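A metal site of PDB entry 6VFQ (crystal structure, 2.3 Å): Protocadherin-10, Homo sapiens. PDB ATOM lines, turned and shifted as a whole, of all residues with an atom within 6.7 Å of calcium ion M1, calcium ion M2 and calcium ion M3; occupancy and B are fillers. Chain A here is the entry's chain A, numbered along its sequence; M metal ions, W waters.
OD1 of Asp 188 sits at hydrogen-bond distance from N of Arg 213 (2.9 Å). O of Asp 133 lies within hydrogen-bond range of OG of Ser 138 (3.2 Å). N of Arg 64 lies close to OE1 of Glu 9, 3.0 Å away. The backbone NH (N) of Glu 9 is in hydrogen-bond range of the backbone carbonyl oxygen (O) of Leu 96. The side-chain amide nitrogen of Asn 101 sits close to the side-chain carboxylate of Glu 65 (3.3 Å). The side-chain carboxylate of Asp 97 is in hydrogen-bond range of the backbone NH of Val 134, at 3.1 Å. The side-chain carboxylate of Asp 97 lies close to the guanidinium group of Arg 64 (3.3 Å). O of Asn 99 is in hydrogen-bond range of NH1 of Arg 213 (3.2 Å).
Within 4 Å of calcium ion M1: Glu 9, Glu 65, Asp 97, Ile 98, Asp 100, Asn 101 and Asp 133.
Five residues have an atom within 4 Å of calcium ion M2: Glu 9, Glu 10, Asp 63, Glu 65 and Asp 100. The nearest printed residue that does not touch calcium ion M2 is Arg 64 (4.2 Å).
Six residues have an atom within 4 Å of calcium ion M3: Asn 99, Asn 101, Asp 131, Asp 133, Asn 137 and Asp 188.
Calcium ion M1 is bound by the side-chain carboxylate (OD1) of Asp 97 (2.2 Å), the side-chain carboxylate (OD1) of Asp 100 (2.2 Å), the backbone carbonyl oxygen (O) of Ile 98 (2.4 Å), the side-chain carboxylate (OE2) of Glu 9 (2.4 Å), the side-chain carboxylate (OD1) of Asp 133 (2.4 Å), the side-chain carboxylate (OE1) of Glu 65 (2.5 Å) and the side-chain carboxylate (OE2) of Glu 65 (2.6 Å).
Calcium ion M2 is bound by OD2 of Asp 100 (2.2 Å), OD1 of Asp 63 (2.3 Å), OE2 of Glu 65 (2.3 Å), water W1 (2.4 Å), OE1 of Glu 9 (2.4 Å) and OE1 of Glu 10 (2.5 Å). Calcium ion M2 has six donor atoms within binding distance.
Calcium ion M3 is bound by the backbone carbonyl oxygen (O) of Asn 101 (2.3 Å), the backbone carbonyl oxygen (O) of Asn 137 (2.3 Å), the side-chain carboxylate (OD2) of Asp 131 (2.4 Å), the side-chain amide oxygen (OD1) of Asn 99 (2.4 Å), the side-chain carboxylate (OD2) of Asp 133 (2.4 Å), the side-chain carboxylate (OD2) of Asp 188 (2.5 Å) and the side-chain carboxylate (OD1) of Asp 131 (2.5 Å).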
ATOM      1  N   GLU A   9     -15.598 -21.729   6.478  1.00  0.00           N
ATOM      2  CA  GLU A   9     -14.245 -22.173   6.784  1.00  0.00           C
ATOM      3  C   GLU A   9     -14.065 -23.586   6.259  1.00  0.00           C
ATOM      4  O   GLU A   9     -15.025 -24.327   6.075  1.00  0.00           O
ATOM      5  CB  GLU A   9     -13.976 -22.138   8.293  1.00  0.00           C
ATOM      6  CG  GLU A   9     -14.801 -23.156   9.067  1.00  0.00           C
ATOM      7  CD  GLU A   9     -14.259 -23.432  10.473  1.00  0.00           C
ATOM      8  OE1 GLU A   9     -13.032 -23.575  10.653  1.00  0.00           O
ATOM      9  OE2 GLU A   9     -15.091 -23.505  11.400  1.00  0.00           O
ATOM     10  N   GLU A  10     -12.814 -23.927   5.978  1.00  0.00           N
ATOM     11  CA  GLU A  10     -12.424 -25.263   5.558  1.00  0.00           C
ATOM     12  C   GLU A  10     -12.890 -25.614   4.136  1.00  0.00           C
ATOM     13  O   GLU A  10     -13.015 -26.793   3.805  1.00  0.00           O
ATOM     14  CB  GLU A  10     -12.931 -26.314   6.553  1.00  0.00           C
ATOM     15  CG  GLU A  10     -12.609 -25.989   8.028  1.00  0.00           C
ATOM     16  CD  GLU A  10     -11.123 -26.020   8.388  1.00  0.00           C
ATOM     17  OE1 GLU A  10     -10.778 -25.588   9.521  1.00  0.00           O
ATOM     18  OE2 GLU A  10     -10.295 -26.496   7.569  1.00  0.00           O
ATOM     19  N   ILE A  62      -9.142 -22.158   4.914  1.00  0.00           N
ATOM     20  CA  ILE A  62      -9.294 -21.290   6.073  1.00  0.00           C
ATOM     21  C   ILE A  62      -9.756 -22.107   7.263  1.00  0.00           C
ATOM     22  O   ILE A  62     -10.816 -22.746   7.209  1.00  0.00           O
ATOM     23  CB  ILE A  62     -10.285 -20.149   5.775  1.00  0.00           C
ATOM     24  CG1 ILE A  62      -9.836 -19.361   4.545  1.00  0.00           C
ATOM     25  CG2 ILE A  62     -10.407 -19.255   7.000  1.00  0.00           C
ATOM     26  CD1 ILE A  62     -10.851 -18.322   4.077  1.00  0.00           C
ATOM     27  N   ASP A  63      -8.961 -22.118   8.330  1.00  0.00           N
ATOM     28  CA  ASP A  63      -9.383 -22.639   9.635  1.00  0.00           C
ATOM     29  C   ASP A  63      -9.765 -21.451  10.499  1.00  0.00           C
ATOM     30  O   ASP A  63      -8.902 -20.673  10.929  1.00  0.00           O
ATOM     31  CB  ASP A  63      -8.293 -23.457  10.303  1.00  0.00           C
ATOM     32  CG  ASP A  63      -8.691 -23.938  11.712  1.00  0.00           C
ATOM     33  OD1 ASP A  63      -9.903 -23.906  12.062  1.00  0.00           O
ATOM     34  OD2 ASP A  63      -7.784 -24.345  12.476  1.00  0.00           O
ATOM     35  N   ARG A  64     -11.062 -21.268  10.704  1.00  0.00           N
ATOM     36  CA  ARG A  64     -11.525 -20.139  11.494  1.00  0.00           C
ATOM     37  C   ARG A  64     -10.936 -20.181  12.895  1.00  0.00           C
ATOM     38  O   ARG A  64     -10.574 -19.139  13.454  1.00  0.00           O
ATOM     39  CB  ARG A  64     -13.056 -20.142  11.563  1.00  0.00           C
ATOM     40  CG  ARG A  64     -13.665 -18.817  12.028  1.00  0.00           C
ATOM     41  CD  ARG A  64     -15.009 -19.059  12.683  1.00  0.00           C
ATOM     42  NE  ARG A  64     -14.750 -19.947  13.817  1.00  0.00           N
ATOM     43  CZ  ARG A  64     -14.275 -19.556  14.994  1.00  0.00           C
ATOM     44  NH1 ARG A  64     -14.058 -18.272  15.243  1.00  0.00           N
ATOM     45  NH2 ARG A  64     -14.024 -20.463  15.925  1.00  0.00           N
ATOM     46  N   GLU A  65     -10.828 -21.380  13.489  1.00  0.00           N
ATOM     47  CA  GLU A  65     -10.320 -21.454  14.853  1.00  0.00           C
ATOM     48  C   GLU A  65      -8.918 -20.902  14.939  1.00  0.00           C
ATOM     49  O   GLU A  65      -8.496 -20.402  15.992  1.00  0.00           O
ATOM     50  CB  GLU A  65     -10.360 -22.891  15.384  1.00  0.00           C
ATOM     51  CG  GLU A  65     -11.754 -23.370  15.788  1.00  0.00           C
ATOM     52  CD  GLU A  65     -12.769 -23.492  14.633  1.00  0.00           C
ATOM     53  OE1 GLU A  65     -13.781 -22.759  14.683  1.00  0.00           O
ATOM     54  OE2 GLU A  65     -12.574 -24.330  13.704  1.00  0.00           O
ATOM     55  N   GLN A  66      -8.174 -20.941  13.836  1.00  0.00           N
ATOM     56  CA  GLN A  66      -6.799 -20.462  13.856  1.00  0.00           C
ATOM     57  C   GLN A  66      -6.725 -18.956  13.668  1.00  0.00           C
ATOM     58  O   GLN A  66      -6.081 -18.255  14.457  1.00  0.00           O
ATOM     59  CB  GLN A  66      -5.974 -21.178  12.801  1.00  0.00           C
ATOM     60  CG  GLN A  66      -4.587 -20.581  12.672  1.00  0.00           C
ATOM     61  CD  GLN A  66      -3.619 -21.562  12.082  1.00  0.00           C
ATOM     62  OE1 GLN A  66      -3.765 -22.763  12.248  1.00  0.00           O
ATOM     63  NE2 GLN A  66      -2.622 -21.049  11.369  1.00  0.00           N
ATOM     64  N   LEU A  96     -17.486 -18.064   8.047  1.00  0.00           N
ATOM     65  CA  LEU A  96     -18.484 -18.679   8.885  1.00  0.00           C
ATOM     66  C   LEU A  96     -17.930 -19.935   9.549  1.00  0.00           C
ATOM     67  O   LEU A  96     -17.266 -20.748   8.896  1.00  0.00           O
ATOM     68  CB  LEU A  96     -19.705 -19.056   8.055  1.00  0.00           C
ATOM     69  CG  LEU A  96     -20.255 -17.907   7.206  1.00  0.00           C
ATOM     70  CD1 LEU A  96     -21.391 -18.395   6.332  1.00  0.00           C
ATOM     71  CD2 LEU A  96     -20.690 -16.755   8.099  1.00  0.00           C
ATOM     72  N   ASP A  97     -18.210 -20.085  10.847  1.00  0.00           N
ATOM     73  CA  ASP A  97     -17.760 -21.238  11.628  1.00  0.00           C
ATOM     74  C   ASP A  97     -18.588 -22.475  11.296  1.00  0.00           C
ATOM     75  O   ASP A  97     -19.818 -22.397  11.218  1.00  0.00           O
ATOM     76  CB  ASP A  97     -17.871 -20.936  13.124  1.00  0.00           C
ATOM     77  CG  ASP A  97     -17.562 -22.148  14.023  1.00  0.00           C
ATOM     78  OD1 ASP A  97     -16.479 -22.790  13.874  1.00  0.00           O
ATOM     79  OD2 ASP A  97     -18.410 -22.435  14.910  1.00  0.00           O
ATOM     80  N   ILE A  98     -17.918 -23.604  11.101  1.00  0.00           N
ATOM     81  CA  ILE A  98     -18.609 -24.892  11.113  1.00  0.00           C
ATOM     82  C   ILE A  98     -18.251 -25.651  12.397  1.00  0.00           C
ATOM     83  O   ILE A  98     -17.317 -25.295  13.120  1.00  0.00           O
ATOM     84  CB  ILE A  98     -18.288 -25.733   9.865  1.00  0.00           C
ATOM     85  CG1 ILE A  98     -16.792 -25.989   9.767  1.00  0.00           C
ATOM     86  CG2 ILE A  98     -18.771 -25.048   8.622  1.00  0.00           C
ATOM     87  CD1 ILE A  98     -16.407 -26.923   8.618  1.00  0.00           C
ATOM     88  N   ASN A  99     -19.004 -26.725  12.653  1.00  0.00           N
ATOM     89  CA  ASN A  99     -18.838 -27.536  13.857  1.00  0.00           C
ATOM     90  C   ASN A  99     -17.868 -28.676  13.581  1.00  0.00           C
ATOM     91  O   ASN A  99     -18.245 -29.850  13.516  1.00  0.00           O
ATOM     92  CB  ASN A  99     -20.170 -28.095  14.331  1.00  0.00           C
ATOM     93  CG  ASN A  99     -20.092 -28.612  15.765  1.00  0.00           C
ATOM     94  OD1 ASN A  99     -19.339 -28.079  16.568  1.00  0.00           O
ATOM     95  ND2 ASN A  99     -20.873 -29.643  16.095  1.00  0.00           N
ATOM     96  N   ASP A 100     -16.594 -28.312  13.422  1.00  0.00           N
ATOM     97  CA  ASP A 100     -15.520 -29.275  13.193  1.00  0.00           C
ATOM     98  C   ASP A 100     -14.702 -29.576  14.450  1.00  0.00           C
ATOM     99  O   ASP A 100     -13.607 -30.141  14.342  1.00  0.00           O
ATOM    100  CB  ASP A 100     -14.611 -28.779  12.056  1.00  0.00           C
ATOM    101  CG  ASP A 100     -14.175 -27.334  12.217  1.00  0.00           C
ATOM    102  OD1 ASP A 100     -14.875 -26.584  12.930  1.00  0.00           O
ATOM    103  OD2 ASP A 100     -13.151 -26.939  11.591  1.00  0.00           O
ATOM    104  N   ASN A 101     -15.194 -29.238  15.654  1.00  0.00           N
ATOM    105  CA  ASN A 101     -14.451 -29.557  16.873  1.00  0.00           C
ATOM    106  C   ASN A 101     -15.409 -30.031  17.957  1.00  0.00           C
ATOM    107  O   ASN A 101     -16.483 -29.402  18.162  1.00  0.00           O
ATOM    108  CB  ASN A 101     -13.639 -28.383  17.414  1.00  0.00           C
ATOM    109  CG  ASN A 101     -12.581 -27.932  16.442  1.00  0.00           C
ATOM    110  OD1 ASN A 101     -11.452 -28.387  16.486  1.00  0.00           O
ATOM    111  ND2 ASN A 101     -12.958 -27.046  15.544  1.00  0.00           N
ATOM    112  N   PRO A 102     -15.066 -31.101  18.664  1.00  0.00           N
ATOM    113  CA  PRO A 102     -15.880 -31.530  19.790  1.00  0.00           C
ATOM    114  C   PRO A 102     -15.510 -30.727  21.020  1.00  0.00           C
ATOM    115  O   PRO A 102     -14.427 -30.126  21.097  1.00  0.00           O
ATOM    116  CB  PRO A 102     -15.492 -33.002  19.956  1.00  0.00           C
ATOM    117  CG  PRO A 102     -14.002 -33.007  19.583  1.00  0.00           C
ATOM    118  CD  PRO A 102     -13.811 -31.871  18.570  1.00  0.00           C
ATOM    119  N   PRO A 103     -16.370 -30.687  22.029  1.00  0.00           N
ATOM    120  CA  PRO A 103     -15.902 -30.271  23.348  1.00  0.00           C
ATOM    121  C   PRO A 103     -14.849 -31.263  23.834  1.00  0.00           C
ATOM    122  O   PRO A 103     -14.869 -32.449  23.482  1.00  0.00           O
ATOM    123  CB  PRO A 103     -17.164 -30.278  24.202  1.00  0.00           C
ATOM    124  CG  PRO A 103     -18.156 -31.056  23.425  1.00  0.00           C
ATOM    125  CD  PRO A 103     -17.810 -30.955  21.999  1.00  0.00           C
ATOM    126  N   ASP A 131     -14.661 -26.078  23.950  1.00  0.00           N
ATOM    127  CA  ASP A 131     -15.019 -26.326  22.551  1.00  0.00           C
ATOM    128  C   ASP A 131     -14.556 -25.130  21.729  1.00  0.00           C
ATOM    129  O   ASP A 131     -15.055 -24.016  21.957  1.00  0.00           O
ATOM    130  CB  ASP A 131     -16.514 -26.532  22.383  1.00  0.00           C
ATOM    131  CG  ASP A 131     -16.891 -27.056  20.995  1.00  0.00           C
ATOM    132  OD1 ASP A 131     -16.352 -26.536  19.995  1.00  0.00           O
ATOM    133  OD2 ASP A 131     -17.710 -27.999  20.918  1.00  0.00           O
ATOM    134  N   PRO A 132     -13.611 -25.288  20.814  1.00  0.00           N
ATOM    135  CA  PRO A 132     -13.042 -24.097  20.146  1.00  0.00           C
ATOM    136  C   PRO A 132     -13.965 -23.442  19.117  1.00  0.00           C
ATOM    137  O   PRO A 132     -13.708 -22.295  18.746  1.00  0.00           O
ATOM    138  CB  PRO A 132     -11.774 -24.642  19.478  1.00  0.00           C
ATOM    139  CG  PRO A 132     -12.071 -26.091  19.251  1.00  0.00           C
ATOM    140  CD  PRO A 132     -12.967 -26.531  20.384  1.00  0.00           C
ATOM    141  N   ASP A 133     -15.003 -24.122  18.632  1.00  0.00           N
ATOM    142  CA  ASP A 133     -15.963 -23.506  17.737  1.00  0.00           C
ATOM    143  C   ASP A 133     -16.699 -22.405  18.484  1.00  0.00           C
ATOM    144  O   ASP A 133     -16.569 -22.281  19.709  1.00  0.00           O
ATOM    145  CB  ASP A 133     -16.948 -24.550  17.222  1.00  0.00           C
ATOM    146  CG  ASP A 133     -16.249 -25.684  16.521  1.00  0.00           C
ATOM    147  OD1 ASP A 133     -15.268 -25.428  15.796  1.00  0.00           O
ATOM    148  OD2 ASP A 133     -16.677 -26.838  16.734  1.00  0.00           O
ATOM    149  N   VAL A 134     -17.482 -21.599  17.762  1.00  0.00           N
ATOM    150  CA  VAL A 134     -18.152 -20.441  18.367  1.00  0.00           C
ATOM    151  C   VAL A 134     -19.661 -20.595  18.268  1.00  0.00           C
ATOM    152  O   VAL A 134     -20.195 -21.456  17.566  1.00  0.00           O
ATOM    153  CB  VAL A 134     -17.709 -19.107  17.741  1.00  0.00           C
ATOM    154  CG1 VAL A 134     -16.301 -18.768  18.161  1.00  0.00           C
ATOM    155  CG2 VAL A 134     -17.818 -19.137  16.188  1.00  0.00           C
ATOM    156  N   THR A 136     -23.454 -21.396  18.615  1.00  0.00           N
ATOM    157  CA  THR A 136     -24.175 -22.643  18.818  1.00  0.00           C
ATOM    158  C   THR A 136     -23.279 -23.858  18.643  1.00  0.00           C
ATOM    159  O   THR A 136     -23.602 -24.931  19.150  1.00  0.00           O
ATOM    160  CB  THR A 136     -25.369 -22.731  17.859  1.00  0.00           C
ATOM    161  OG1 THR A 136     -26.234 -23.794  18.270  1.00  0.00           O
ATOM    162  CG2 THR A 136     -24.919 -23.005  16.439  1.00  0.00           C
ATOM    163  N   ASN A 137     -22.168 -23.734  17.911  1.00  0.00           N
ATOM    164  CA  ASN A 137     -21.246 -24.843  17.737  1.00  0.00           C
ATOM    165  C   ASN A 137     -20.359 -25.085  18.946  1.00  0.00           C
ATOM    166  O   ASN A 137     -19.601 -26.073  18.964  1.00  0.00           O
ATOM    167  CB  ASN A 137     -20.384 -24.592  16.502  1.00  0.00           C
ATOM    168  CG  ASN A 137     -21.196 -24.656  15.249  1.00  0.00           C
ATOM    169  OD1 ASN A 137     -22.155 -25.426  15.160  1.00  0.00           O
ATOM    170  ND2 ASN A 137     -20.826 -23.840  14.259  1.00  0.00           N
ATOM    171  N   SER A 138     -20.405 -24.203  19.930  1.00  0.00           N
ATOM    172  CA  SER A 138     -19.601 -24.350  21.133  1.00  0.00           C
ATOM    173  C   SER A 138     -20.325 -25.188  22.182  1.00  0.00           C
ATOM    174  O   SER A 138     -21.426 -25.695  21.971  1.00  0.00           O
ATOM    175  CB  SER A 138     -19.239 -22.984  21.694  1.00  0.00           C
ATOM    176  OG  SER A 138     -18.041 -23.073  22.462  1.00  0.00           O
ATOM    177  N   LEU A 139     -19.683 -25.317  23.341  1.00  0.00           N
ATOM    178  CA  LEU A 139     -20.202 -26.121  24.429  1.00  0.00           C
ATOM    179  C   LEU A 139     -21.614 -25.701  24.813  1.00  0.00           C
ATOM    180  O   LEU A 139     -21.893 -24.516  24.982  1.00  0.00           O
ATOM    181  CB  LEU A 139     -19.251 -25.984  25.615  1.00  0.00           C
ATOM    182  CG  LEU A 139     -19.649 -26.711  26.891  1.00  0.00           C
ATOM    183  CD1 LEU A 139     -19.526 -28.219  26.689  1.00  0.00           C
ATOM    184  CD2 LEU A 139     -18.733 -26.222  27.994  1.00  0.00           C
ATOM    185  N   ASP A 188     -21.785 -30.065  22.448  1.00  0.00           N
ATOM    186  CA  ASP A 188     -21.949 -28.728  21.913  1.00  0.00           C
ATOM    187  C   ASP A 188     -23.364 -28.617  21.351  1.00  0.00           C
ATOM    188  O   ASP A 188     -24.204 -29.488  21.574  1.00  0.00           O
ATOM    189  CB  ASP A 188     -20.852 -28.407  20.886  1.00  0.00           C
ATOM    190  CG  ASP A 188     -20.851 -29.349  19.672  1.00  0.00           C
ATOM    191  OD1 ASP A 188     -21.872 -30.014  19.388  1.00  0.00           O
ATOM    192  OD2 ASP A 188     -19.816 -29.390  18.975  1.00  0.00           O
ATOM    193  N   GLY A 189     -23.642 -27.538  20.619  1.00  0.00           N
ATOM    194  CA  GLY A 189     -25.008 -27.255  20.199  1.00  0.00           C
ATOM    195  C   GLY A 189     -25.260 -27.418  18.713  1.00  0.00           C
ATOM    196  O   GLY A 189     -26.089 -26.690  18.157  1.00  0.00           O
ATOM    197  N   GLY A 190     -24.582 -28.353  18.063  1.00  0.00           N
ATOM    198  CA  GLY A 190     -24.779 -28.562  16.651  1.00  0.00           C
ATOM    199  C   GLY A 190     -25.841 -29.599  16.332  1.00  0.00           C
ATOM    200  O   GLY A 190     -25.542 -30.797  16.259  1.00  0.00           O
ATOM    201  N   ARG A 213     -21.447 -32.707  18.395  1.00  0.00           N
ATOM    202  CA  ARG A 213     -20.239 -33.410  18.805  1.00  0.00           C
ATOM    203  C   ARG A 213     -20.167 -33.491  20.323  1.00  0.00           C
ATOM    204  O   ARG A 213     -20.774 -32.694  21.048  1.00  0.00           O
ATOM    205  CB  ARG A 213     -19.008 -32.728  18.212  1.00  0.00           C
ATOM    206  CG  ARG A 213     -19.171 -32.506  16.711  1.00  0.00           C
ATOM    207  CD  ARG A 213     -17.917 -31.985  16.009  1.00  0.00           C
ATOM    208  NE  ARG A 213     -17.099 -33.091  15.533  1.00  0.00           N
ATOM    209  CZ  ARG A 213     -17.095 -33.565  14.299  1.00  0.00           C
ATOM    210  NH1 ARG A 213     -17.861 -33.020  13.366  1.00  0.00           N
ATOM    211  NH2 ARG A 213     -16.308 -34.587  13.986  1.00  0.00           N
HETATM  212 CA    CA M   1     -15.146 -24.488  13.571  1.00  0.00          CA
HETATM  213 CA    CA M   2     -11.713 -25.238  11.812  1.00  0.00          CA
HETATM  214 CA    CA M   3     -18.018 -27.756  18.556  1.00  0.00          CA
HETATM  215  O   HOH W   1     -10.782 -26.940  13.236  1.00  0.00           O
